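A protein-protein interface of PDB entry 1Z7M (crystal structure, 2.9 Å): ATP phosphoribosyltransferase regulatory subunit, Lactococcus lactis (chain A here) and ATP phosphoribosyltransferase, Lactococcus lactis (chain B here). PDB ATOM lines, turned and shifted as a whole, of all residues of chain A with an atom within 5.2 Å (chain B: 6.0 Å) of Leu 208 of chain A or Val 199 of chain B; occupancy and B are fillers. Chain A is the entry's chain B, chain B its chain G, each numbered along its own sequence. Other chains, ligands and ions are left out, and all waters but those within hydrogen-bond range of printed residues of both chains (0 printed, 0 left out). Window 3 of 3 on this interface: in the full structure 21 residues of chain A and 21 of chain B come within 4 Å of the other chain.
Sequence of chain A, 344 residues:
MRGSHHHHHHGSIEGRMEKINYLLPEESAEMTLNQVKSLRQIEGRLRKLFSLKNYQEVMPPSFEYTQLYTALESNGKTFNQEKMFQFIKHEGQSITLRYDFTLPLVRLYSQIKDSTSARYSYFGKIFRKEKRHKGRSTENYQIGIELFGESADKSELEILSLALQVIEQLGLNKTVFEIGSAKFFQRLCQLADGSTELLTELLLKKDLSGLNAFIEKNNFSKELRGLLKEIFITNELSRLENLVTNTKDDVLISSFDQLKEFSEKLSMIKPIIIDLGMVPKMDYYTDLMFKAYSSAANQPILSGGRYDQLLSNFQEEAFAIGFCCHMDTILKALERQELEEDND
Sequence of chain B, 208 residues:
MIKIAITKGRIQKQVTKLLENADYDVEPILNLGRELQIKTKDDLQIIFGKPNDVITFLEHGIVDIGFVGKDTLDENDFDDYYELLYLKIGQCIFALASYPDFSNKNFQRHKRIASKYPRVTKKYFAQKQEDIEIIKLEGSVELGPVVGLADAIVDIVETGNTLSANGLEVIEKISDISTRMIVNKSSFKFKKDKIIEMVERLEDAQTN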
ATOM      1  N   LYS A 206      -4.557  14.273 -11.613  1.00  0.00           N
ATOM      2  CA  LYS A 206      -4.398  12.839 -11.552  1.00  0.00           C
ATOM      3  C   LYS A 206      -3.933  12.530 -10.159  1.00  0.00           C
ATOM      4  O   LYS A 206      -2.963  11.805  -9.902  1.00  0.00           O
ATOM      5  CB  LYS A 206      -3.434  12.325 -12.610  1.00  0.00           C
ATOM      6  CG  LYS A 206      -3.977  12.472 -14.022  1.00  0.00           C
ATOM      7  CD  LYS A 206      -3.216  11.608 -15.006  1.00  0.00           C
ATOM      8  CE  LYS A 206      -3.767  11.763 -16.407  1.00  0.00           C
ATOM      9  NZ  LYS A 206      -5.244  11.614 -16.435  1.00  0.00           N
ATOM     10  N   ASP A 207      -4.665  13.156  -9.273  1.00  0.00           N
ATOM     11  CA  ASP A 207      -4.443  13.074  -7.865  1.00  0.00           C
ATOM     12  C   ASP A 207      -4.840  11.631  -7.357  1.00  0.00           C
ATOM     13  O   ASP A 207      -5.812  11.500  -6.613  1.00  0.00           O
ATOM     14  CB  ASP A 207      -5.213  14.176  -7.135  1.00  0.00           C
ATOM     15  CG  ASP A 207      -4.828  14.286  -5.673  1.00  0.00           C
ATOM     16  OD1 ASP A 207      -4.273  13.308  -5.130  1.00  0.00           O
ATOM     17  OD2 ASP A 207      -5.080  15.351  -5.071  1.00  0.00           O
ATOM     18  N   LEU A 208      -4.068  10.551  -7.719  1.00  0.00           N
ATOM     19  CA  LEU A 208      -4.318   9.116  -7.330  1.00  0.00           C
ATOM     20  C   LEU A 208      -4.559   8.912  -5.846  1.00  0.00           C
ATOM     21  O   LEU A 208      -5.442   8.145  -5.451  1.00  0.00           O
ATOM     22  CB  LEU A 208      -3.148   8.225  -7.747  1.00  0.00           C
ATOM     23  CG  LEU A 208      -2.789   8.245  -9.247  1.00  0.00           C
ATOM     24  CD1 LEU A 208      -1.614   7.322  -9.554  1.00  0.00           C
ATOM     25  CD2 LEU A 208      -4.001   7.878 -10.086  1.00  0.00           C
ATOM     26  N   SER A 209      -3.768   9.607  -5.037  1.00  0.00           N
ATOM     27  CA  SER A 209      -3.891   9.521  -3.602  1.00  0.00           C
ATOM     28  C   SER A 209      -5.158  10.221  -3.110  1.00  0.00           C
ATOM     29  O   SER A 209      -5.850   9.750  -2.197  1.00  0.00           O
ATOM     30  CB  SER A 209      -2.653  10.134  -2.963  1.00  0.00           C
ATOM     31  OG  SER A 209      -2.667   9.955  -1.555  1.00  0.00           O
ATOM     32  N   GLY A 210      -5.463  11.354  -3.722  1.00  0.00           N
ATOM     33  CA  GLY A 210      -6.647  12.084  -3.338  1.00  0.00           C
ATOM     34  C   GLY A 210      -7.863  11.317  -3.798  1.00  0.00           C
ATOM     35  O   GLY A 210      -8.881  11.288  -3.128  1.00  0.00           O
ATOM     36  N   LEU A 211      -7.764  10.689  -4.957  1.00  0.00           N
ATOM     37  CA  LEU A 211      -8.883   9.923  -5.478  1.00  0.00           C
ATOM     38  C   LEU A 211      -9.210   8.752  -4.570  1.00  0.00           C
ATOM     39  O   LEU A 211     -10.367   8.427  -4.371  1.00  0.00           O
ATOM     40  CB  LEU A 211      -8.541   9.394  -6.862  1.00  0.00           C
ATOM     41  CG  LEU A 211      -9.482   8.350  -7.444  1.00  0.00           C
ATOM     42  CD1 LEU A 211     -10.840   8.958  -7.607  1.00  0.00           C
ATOM     43  CD2 LEU A 211      -8.949   7.853  -8.773  1.00  0.00           C
ATOM     44  N   ASN A 212      -8.178   8.116  -4.028  1.00  0.00           N
ATOM     45  CA  ASN A 212      -8.360   6.975  -3.166  1.00  0.00           C
ATOM     46  C   ASN A 212      -9.129   7.399  -1.945  1.00  0.00           C
ATOM     47  O   ASN A 212     -10.092   6.747  -1.557  1.00  0.00           O
ATOM     48  CB  ASN A 212      -7.009   6.349  -2.815  1.00  0.00           C
ATOM     49  CG  ASN A 212      -7.152   5.012  -2.114  1.00  0.00           C
ATOM     50  N   LYS A 229     -10.659   4.499 -10.591  1.00  0.00           N
ATOM     51  CA  LYS A 229      -9.237   4.207 -10.388  1.00  0.00           C
ATOM     52  C   LYS A 229      -8.466   3.999 -11.693  1.00  0.00           C
ATOM     53  O   LYS A 229      -7.286   4.329 -11.784  1.00  0.00           O
ATOM     54  CB  LYS A 229      -9.062   2.935  -9.558  1.00  0.00           C
ATOM     55  CG  LYS A 229      -9.525   2.999  -8.134  1.00  0.00           C
ATOM     56  CD  LYS A 229      -9.209   1.674  -7.416  1.00  0.00           C
ATOM     57  CE  LYS A 229      -9.618   1.697  -5.939  1.00  0.00           C
ATOM     58  NZ  LYS A 229      -8.918   2.776  -5.159  1.00  0.00           N
ATOM     59  N   PHE A 232      -7.897   7.003 -14.765  1.00  0.00           N
ATOM     60  CA  PHE A 232      -6.860   7.950 -14.391  1.00  0.00           C
ATOM     61  C   PHE A 232      -5.518   7.572 -14.981  1.00  0.00           C
ATOM     62  O   PHE A 232      -4.669   8.433 -15.137  1.00  0.00           O
ATOM     63  CB  PHE A 232      -6.678   7.987 -12.879  1.00  0.00           C
ATOM     64  CG  PHE A 232      -7.479   9.038 -12.176  1.00  0.00           C
ATOM     65  CD1 PHE A 232      -8.856   9.121 -12.342  1.00  0.00           C
ATOM     66  CD2 PHE A 232      -6.859   9.898 -11.281  1.00  0.00           C
ATOM     67  CE1 PHE A 232      -9.596  10.041 -11.622  1.00  0.00           C
ATOM     68  CE2 PHE A 232      -7.593  10.818 -10.562  1.00  0.00           C
ATOM     69  CZ  PHE A 232      -8.960  10.891 -10.730  1.00  0.00           C
ATOM     70  N   ILE A 233      -5.306   6.294 -15.296  1.00  0.00           N
ATOM     71  CA  ILE A 233      -4.000   5.882 -15.802  1.00  0.00           C
ATOM     72  C   ILE A 233      -3.911   4.928 -16.980  1.00  0.00           C
ATOM     73  O   ILE A 233      -2.847   4.343 -17.191  1.00  0.00           O
ATOM     74  CB  ILE A 233      -3.141   5.256 -14.677  1.00  0.00           C
ATOM     75  CG1 ILE A 233      -3.760   3.936 -14.229  1.00  0.00           C
ATOM     76  CG2 ILE A 233      -3.021   6.217 -13.500  1.00  0.00           C
ATOM     77  CD1 ILE A 233      -2.955   3.220 -13.162  1.00  0.00           C
ATOM     78  N   TYR B  24      14.828   0.781  -4.584  1.00  0.00           N
ATOM     79  CA  TYR B  24      15.541   1.604  -5.558  1.00  0.00           C
ATOM     80  C   TYR B  24      16.954   1.932  -5.068  1.00  0.00           C
ATOM     81  O   TYR B  24      17.164   2.237  -3.892  1.00  0.00           O
ATOM     82  CB  TYR B  24      14.771   2.897  -5.817  1.00  0.00           C
ATOM     83  CG  TYR B  24      13.595   2.777  -6.767  1.00  0.00           C
ATOM     84  CD1 TYR B  24      12.287   2.719  -6.297  1.00  0.00           C
ATOM     85  CD2 TYR B  24      13.787   2.812  -8.141  1.00  0.00           C
ATOM     86  CE1 TYR B  24      11.200   2.711  -7.182  1.00  0.00           C
ATOM     87  CE2 TYR B  24      12.713   2.803  -9.025  1.00  0.00           C
ATOM     88  CZ  TYR B  24      11.433   2.757  -8.540  1.00  0.00           C
ATOM     89  OH  TYR B  24      10.398   2.791  -9.424  1.00  0.00           O
ATOM     90  N   GLU B  83      -0.373  15.333  -9.740  1.00  0.00           N
ATOM     91  CA  GLU B  83       0.044  15.065  -8.375  1.00  0.00           C
ATOM     92  C   GLU B  83      -0.276  13.583  -8.213  1.00  0.00           C
ATOM     93  O   GLU B  83      -1.340  13.212  -7.713  1.00  0.00           O
ATOM     94  CB  GLU B  83      -0.766  15.914  -7.395  1.00  0.00           C
ATOM     95  CG  GLU B  83      -0.009  16.311  -6.130  1.00  0.00           C
ATOM     96  CD  GLU B  83      -0.757  17.360  -5.306  1.00  0.00           C
ATOM     97  OE1 GLU B  83      -1.785  16.998  -4.675  1.00  0.00           O
ATOM     98  OE2 GLU B  83      -0.330  18.549  -5.296  1.00  0.00           O
ATOM     99  N   LEU B  84       0.647  12.742  -8.676  1.00  0.00           N
ATOM    100  CA  LEU B  84       0.466  11.301  -8.632  1.00  0.00           C
ATOM    101  C   LEU B  84       0.551  10.701  -7.252  1.00  0.00           C
ATOM    102  O   LEU B  84      -0.395  10.071  -6.788  1.00  0.00           O
ATOM    103  CB  LEU B  84       1.466  10.600  -9.554  1.00  0.00           C
ATOM    104  CG  LEU B  84       1.313  10.871 -11.055  1.00  0.00           C
ATOM    105  CD1 LEU B  84       2.091   9.806 -11.827  1.00  0.00           C
ATOM    106  CD2 LEU B  84      -0.158  10.839 -11.468  1.00  0.00           C
ATOM    107  N   LEU B  85       1.673  10.888  -6.581  1.00  0.00           N
ATOM    108  CA  LEU B  85       1.807  10.327  -5.247  1.00  0.00           C
ATOM    109  C   LEU B  85       1.802  11.382  -4.153  1.00  0.00           C
ATOM    110  O   LEU B  85       2.270  12.506  -4.339  1.00  0.00           O
ATOM    111  CB  LEU B  85       3.082   9.494  -5.146  1.00  0.00           C
ATOM    112  CG  LEU B  85       3.133   8.701  -3.846  1.00  0.00           C
ATOM    113  CD1 LEU B  85       2.014   7.674  -3.842  1.00  0.00           C
ATOM    114  CD2 LEU B  85       4.479   8.030  -3.707  1.00  0.00           C
ATOM    115  N   MET B 181       4.532  14.118  -4.807  1.00  0.00           N
ATOM    116  CA  MET B 181       5.288  13.762  -5.997  1.00  0.00           C
ATOM    117  C   MET B 181       4.538  14.283  -7.203  1.00  0.00           C
ATOM    118  O   MET B 181       3.461  13.791  -7.515  1.00  0.00           O
ATOM    119  CB  MET B 181       5.438  12.246  -6.115  1.00  0.00           C
ATOM    120  CG  MET B 181       6.042  11.806  -7.444  1.00  0.00           C
ATOM    121  SD  MET B 181       6.168  10.012  -7.634  1.00  0.00           S
ATOM    122  CE  MET B 181       4.573   9.590  -8.274  1.00  0.00           C
ATOM    123  N   LYS B 194       7.078   3.394 -16.792  1.00  0.00           N
ATOM    124  CA  LYS B 194       7.961   3.609 -15.656  1.00  0.00           C
ATOM    125  C   LYS B 194       7.391   4.581 -14.649  1.00  0.00           C
ATOM    126  O   LYS B 194       7.664   4.456 -13.454  1.00  0.00           O
ATOM    127  CB  LYS B 194       9.318   4.113 -16.145  1.00  0.00           C
ATOM    128  CG  LYS B 194       9.906   3.285 -17.283  1.00  0.00           C
ATOM    129  CD  LYS B 194      10.068   1.821 -16.889  1.00  0.00           C
ATOM    130  CE  LYS B 194      10.583   1.006 -18.055  1.00  0.00           C
ATOM    131  NZ  LYS B 194      11.835   1.607 -18.609  1.00  0.00           N
ATOM    132  N   ILE B 195       6.607   5.548 -15.122  1.00  0.00           N
ATOM    133  CA  ILE B 195       6.029   6.522 -14.210  1.00  0.00           C
ATOM    134  C   ILE B 195       5.028   5.820 -13.306  1.00  0.00           C
ATOM    135  O   ILE B 195       5.154   5.886 -12.083  1.00  0.00           O
ATOM    136  CB  ILE B 195       5.324   7.696 -14.953  1.00  0.00           C
ATOM    137  CG1 ILE B 195       6.308   8.425 -15.876  1.00  0.00           C
ATOM    138  CG2 ILE B 195       4.780   8.709 -13.929  1.00  0.00           C
ATOM    139  CD1 ILE B 195       7.294   9.307 -15.159  1.00  0.00           C
ATOM    140  N   ILE B 196       4.051   5.133 -13.896  1.00  0.00           N
ATOM    141  CA  ILE B 196       3.056   4.423 -13.099  1.00  0.00           C
ATOM    142  C   ILE B 196       3.743   3.408 -12.202  1.00  0.00           C
ATOM    143  O   ILE B 196       3.402   3.271 -11.027  1.00  0.00           O
ATOM    144  CB  ILE B 196       2.013   3.692 -13.977  1.00  0.00           C
ATOM    145  CG1 ILE B 196       1.121   4.710 -14.683  1.00  0.00           C
ATOM    146  CG2 ILE B 196       1.142   2.790 -13.120  1.00  0.00           C
ATOM    147  CD1 ILE B 196       0.468   5.702 -13.725  1.00  0.00           C
ATOM    148  N   GLU B 197       4.728   2.711 -12.758  1.00  0.00           N
ATOM    149  CA  GLU B 197       5.492   1.714 -12.015  1.00  0.00           C
ATOM    150  C   GLU B 197       6.094   2.296 -10.723  1.00  0.00           C
ATOM    151  O   GLU B 197       5.826   1.801  -9.633  1.00  0.00           O
ATOM    152  CB  GLU B 197       6.594   1.143 -12.916  1.00  0.00           C
ATOM    153  CG  GLU B 197       7.278  -0.109 -12.376  1.00  0.00           C
ATOM    154  CD  GLU B 197       7.658  -1.084 -13.487  1.00  0.00           C
ATOM    155  OE1 GLU B 197       8.437  -0.689 -14.393  1.00  0.00           O
ATOM    156  OE2 GLU B 197       7.170  -2.243 -13.455  1.00  0.00           O
ATOM    157  N   MET B 198       6.891   3.350 -10.841  1.00  0.00           N
ATOM    158  CA  MET B 198       7.490   3.950  -9.654  1.00  0.00           C
ATOM    159  C   MET B 198       6.443   4.397  -8.660  1.00  0.00           C
ATOM    160  O   MET B 198       6.683   4.383  -7.450  1.00  0.00           O
ATOM    161  CB  MET B 198       8.345   5.162 -10.001  1.00  0.00           C
ATOM    162  CG  MET B 198       9.023   5.762  -8.767  1.00  0.00           C
ATOM    163  SD  MET B 198      10.135   7.092  -9.176  1.00  0.00           S
ATOM    164  CE  MET B 198      11.006   6.372 -10.588  1.00  0.00           C
ATOM    165  N   VAL B 199       5.292   4.816  -9.181  1.00  0.00           N
ATOM    166  CA  VAL B 199       4.195   5.265  -8.340  1.00  0.00           C
ATOM    167  C   VAL B 199       3.744   4.100  -7.463  1.00  0.00           C
ATOM    168  O   VAL B 199       3.674   4.225  -6.239  1.00  0.00           O
ATOM    169  CB  VAL B 199       3.028   5.783  -9.200  1.00  0.00           C
ATOM    170  CG1 VAL B 199       1.899   6.274  -8.322  1.00  0.00           C
ATOM    171  CG2 VAL B 199       3.509   6.906 -10.068  1.00  0.00           C
ATOM    172  N   GLU B 200       3.461   2.961  -8.094  1.00  0.00           N
ATOM    173  CA  GLU B 200       3.044   1.765  -7.361  1.00  0.00           C
ATOM    174  C   GLU B 200       4.080   1.496  -6.262  1.00  0.00           C
ATOM    175  O   GLU B 200       3.769   1.550  -5.071  1.00  0.00           O
ATOM    176  CB  GLU B 200       2.994   0.542  -8.284  1.00  0.00           C
ATOM    177  CG  GLU B 200       2.264   0.716  -9.620  1.00  0.00           C
ATOM    178  CD  GLU B 200       0.763   0.918  -9.475  1.00  0.00           C
ATOM    179  OE1 GLU B 200       0.051   0.858 -10.513  1.00  0.00           O
ATOM    180  OE2 GLU B 200       0.299   1.145  -8.330  1.00  0.00           O
ATOM    181  N   ARG B 201       5.314   1.223  -6.675  1.00  0.00           N
ATOM    182  CA  ARG B 201       6.408   0.930  -5.752  1.00  0.00           C
ATOM    183  C   ARG B 201       6.556   1.876  -4.557  1.00  0.00           C
ATOM    184  O   ARG B 201       6.805   1.423  -3.439  1.00  0.00           O
ATOM    185  CB  ARG B 201       7.728   0.859  -6.531  1.00  0.00           C
ATOM    186  CG  ARG B 201       7.754  -0.277  -7.549  1.00  0.00           C
ATOM    187  CD  ARG B 201       9.059  -0.358  -8.316  1.00  0.00           C
ATOM    188  NE  ARG B 201      10.196  -0.589  -7.437  1.00  0.00           N
ATOM    189  CZ  ARG B 201      11.447  -0.693  -7.866  1.00  0.00           C
ATOM    190  NH1 ARG B 201      11.711  -0.587  -9.160  1.00  0.00           N
ATOM    191  NH2 ARG B 201      12.431  -0.896  -7.004  1.00  0.00           N
ATOM    192  N   LEU B 202       6.416   3.179  -4.786  1.00  0.00           N
ATOM    193  CA  LEU B 202       6.536   4.155  -3.704  1.00  0.00           C
ATOM    194  C   LEU B 202       5.289   4.141  -2.845  1.00  0.00           C
ATOM    195  O   LEU B 202       5.337   4.472  -1.658  1.00  0.00           O
ATOM    196  CB  LEU B 202       6.716   5.563  -4.258  1.00  0.00           C
ATOM    197  CG  LEU B 202       8.056   5.906  -4.886  1.00  0.00           C
ATOM    198  CD1 LEU B 202       8.031   7.344  -5.391  1.00  0.00           C
ATOM    199  CD2 LEU B 202       9.145   5.708  -3.852  1.00  0.00           C
ATOM    200  N   GLU B 203       4.171   3.764  -3.464  1.00  0.00           N
ATOM    201  CA  GLU B 203       2.886   3.708  -2.782  1.00  0.00           C
ATOM    202  C   GLU B 203       2.925   2.685  -1.655  1.00  0.00           C
ATOM    203  O   GLU B 203       2.542   2.981  -0.529  1.00  0.00           O
ATOM    204  CB  GLU B 203       1.770   3.350  -3.774  1.00  0.00           C
ATOM    205  CG  GLU B 203       0.403   3.959  -3.430  1.00  0.00           C
ATOM    206  CD  GLU B 203      -0.736   3.511  -4.376  1.00  0.00           C
ATOM    207  OE1 GLU B 203      -0.534   3.467  -5.620  1.00  0.00           O
ATOM    208  OE2 GLU B 203      -1.849   3.225  -3.862  1.00  0.00           O
ATOM    209  N   ASP B 204       3.401   1.483  -1.960  1.00  0.00           N
ATOM    210  CA  ASP B 204       3.487   0.422  -0.969  1.00  0.00           C
ATOM    211  C   ASP B 204       4.557   0.697   0.081  1.00  0.00           C
ATOM    212  O   ASP B 204       4.506   0.152   1.182  1.00  0.00           O
ATOM    213  CB  ASP B 204       3.782  -0.901  -1.657  1.00  0.00           C
ATOM    214  CG  ASP B 204       2.855  -1.161  -2.811  1.00  0.00           C
ATOM    215  OD1 ASP B 204       1.661  -0.802  -2.705  1.00  0.00           O
ATOM    216  OD2 ASP B 204       3.317  -1.725  -3.824  1.00  0.00           O
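Printed residues of chain B within 4 Å of Asp 207 of chain A: Glu 83.
Printed residues of chain B within 4 Å of Ser 209 of chain A: Leu 84 (3.8 Å).
Gly 210 of chain A touches none of the printed residues of chain B.
Of the printed residues of chain B, Ile 233 of chain A touches Ile 196 (3.5 Å).
Printed residues of chain A within 4 Å of Glu 83 of chain B: Lys 206, Asp 207 and Leu 208.
Of chain A, only Leu 208 (3.9 Å) comes within 4 Å of Val 199 of chain B.
Asp 204 of chain B touches none of the printed residues of chain A.
The nearest residue of chain B that does not touch Leu 208 of chain A is Ile 196 of chain B (4.9 Å).
The nearest printed residue of chain A that does not touch Glu 83 of chain B is Ser 209 of chain A (5.1 Å).
NZ of Lys 206 of chain A sits at hydrogen-bond distance from O of Phe 232 of chain A (3.5 Å).
The backbone NH of Gly 210 of chain A is in hydrogen-bond range of the side-chain carboxylate of Asp 207 of chain A (2.7 Å).
The backbone carbonyl oxygen (O) of Met 181 of chain B sits at hydrogen-bond distance from the backbone NH (N) of Leu 84 of chain B (3.2 Å).
Hydrophobic or aromatic side chains of chain A that line the printed part of chain B: Leu 208 and Ile 233.
Of the 16 printed residues of chain B, 4 touch a printed residue of chain A.
Among the printed residues, 8 pairs touch across the chains.
Among the printed residues, no Asp or Glu carboxylate lies within 4 Å of a Lys or Arg side-chain nitrogen of the other chain.
CD2 of Leu 84 of chain B touches O of Lys 206 of chain A, 3.4 Å away.
Glu 83 of chain B touches Asp 207 of chain A (O to CA, 3.1 Å).
Glu 83 of chain B touches Leu 208 of chain A (O to N, 3.8 Å).
Leu 84 of chain B touches Leu 208 of chain A.
CD1 of Leu 208 of chain A touches CG1 of Val 199 of chain B (3.9 Å).
Ser 209 of chain A touches Leu 84 of chain B (N to O, 3.8 Å).
CG2 of Ile 233 of chain A touches CD1 of Ile 196 of chain B, at 3.5 Å.
The backbone carbonyl oxygen (O) of Lys 206 of chain A lies close to the backbone carbonyl oxygen (O) of Glu 83 of chain B (3.1 Å).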
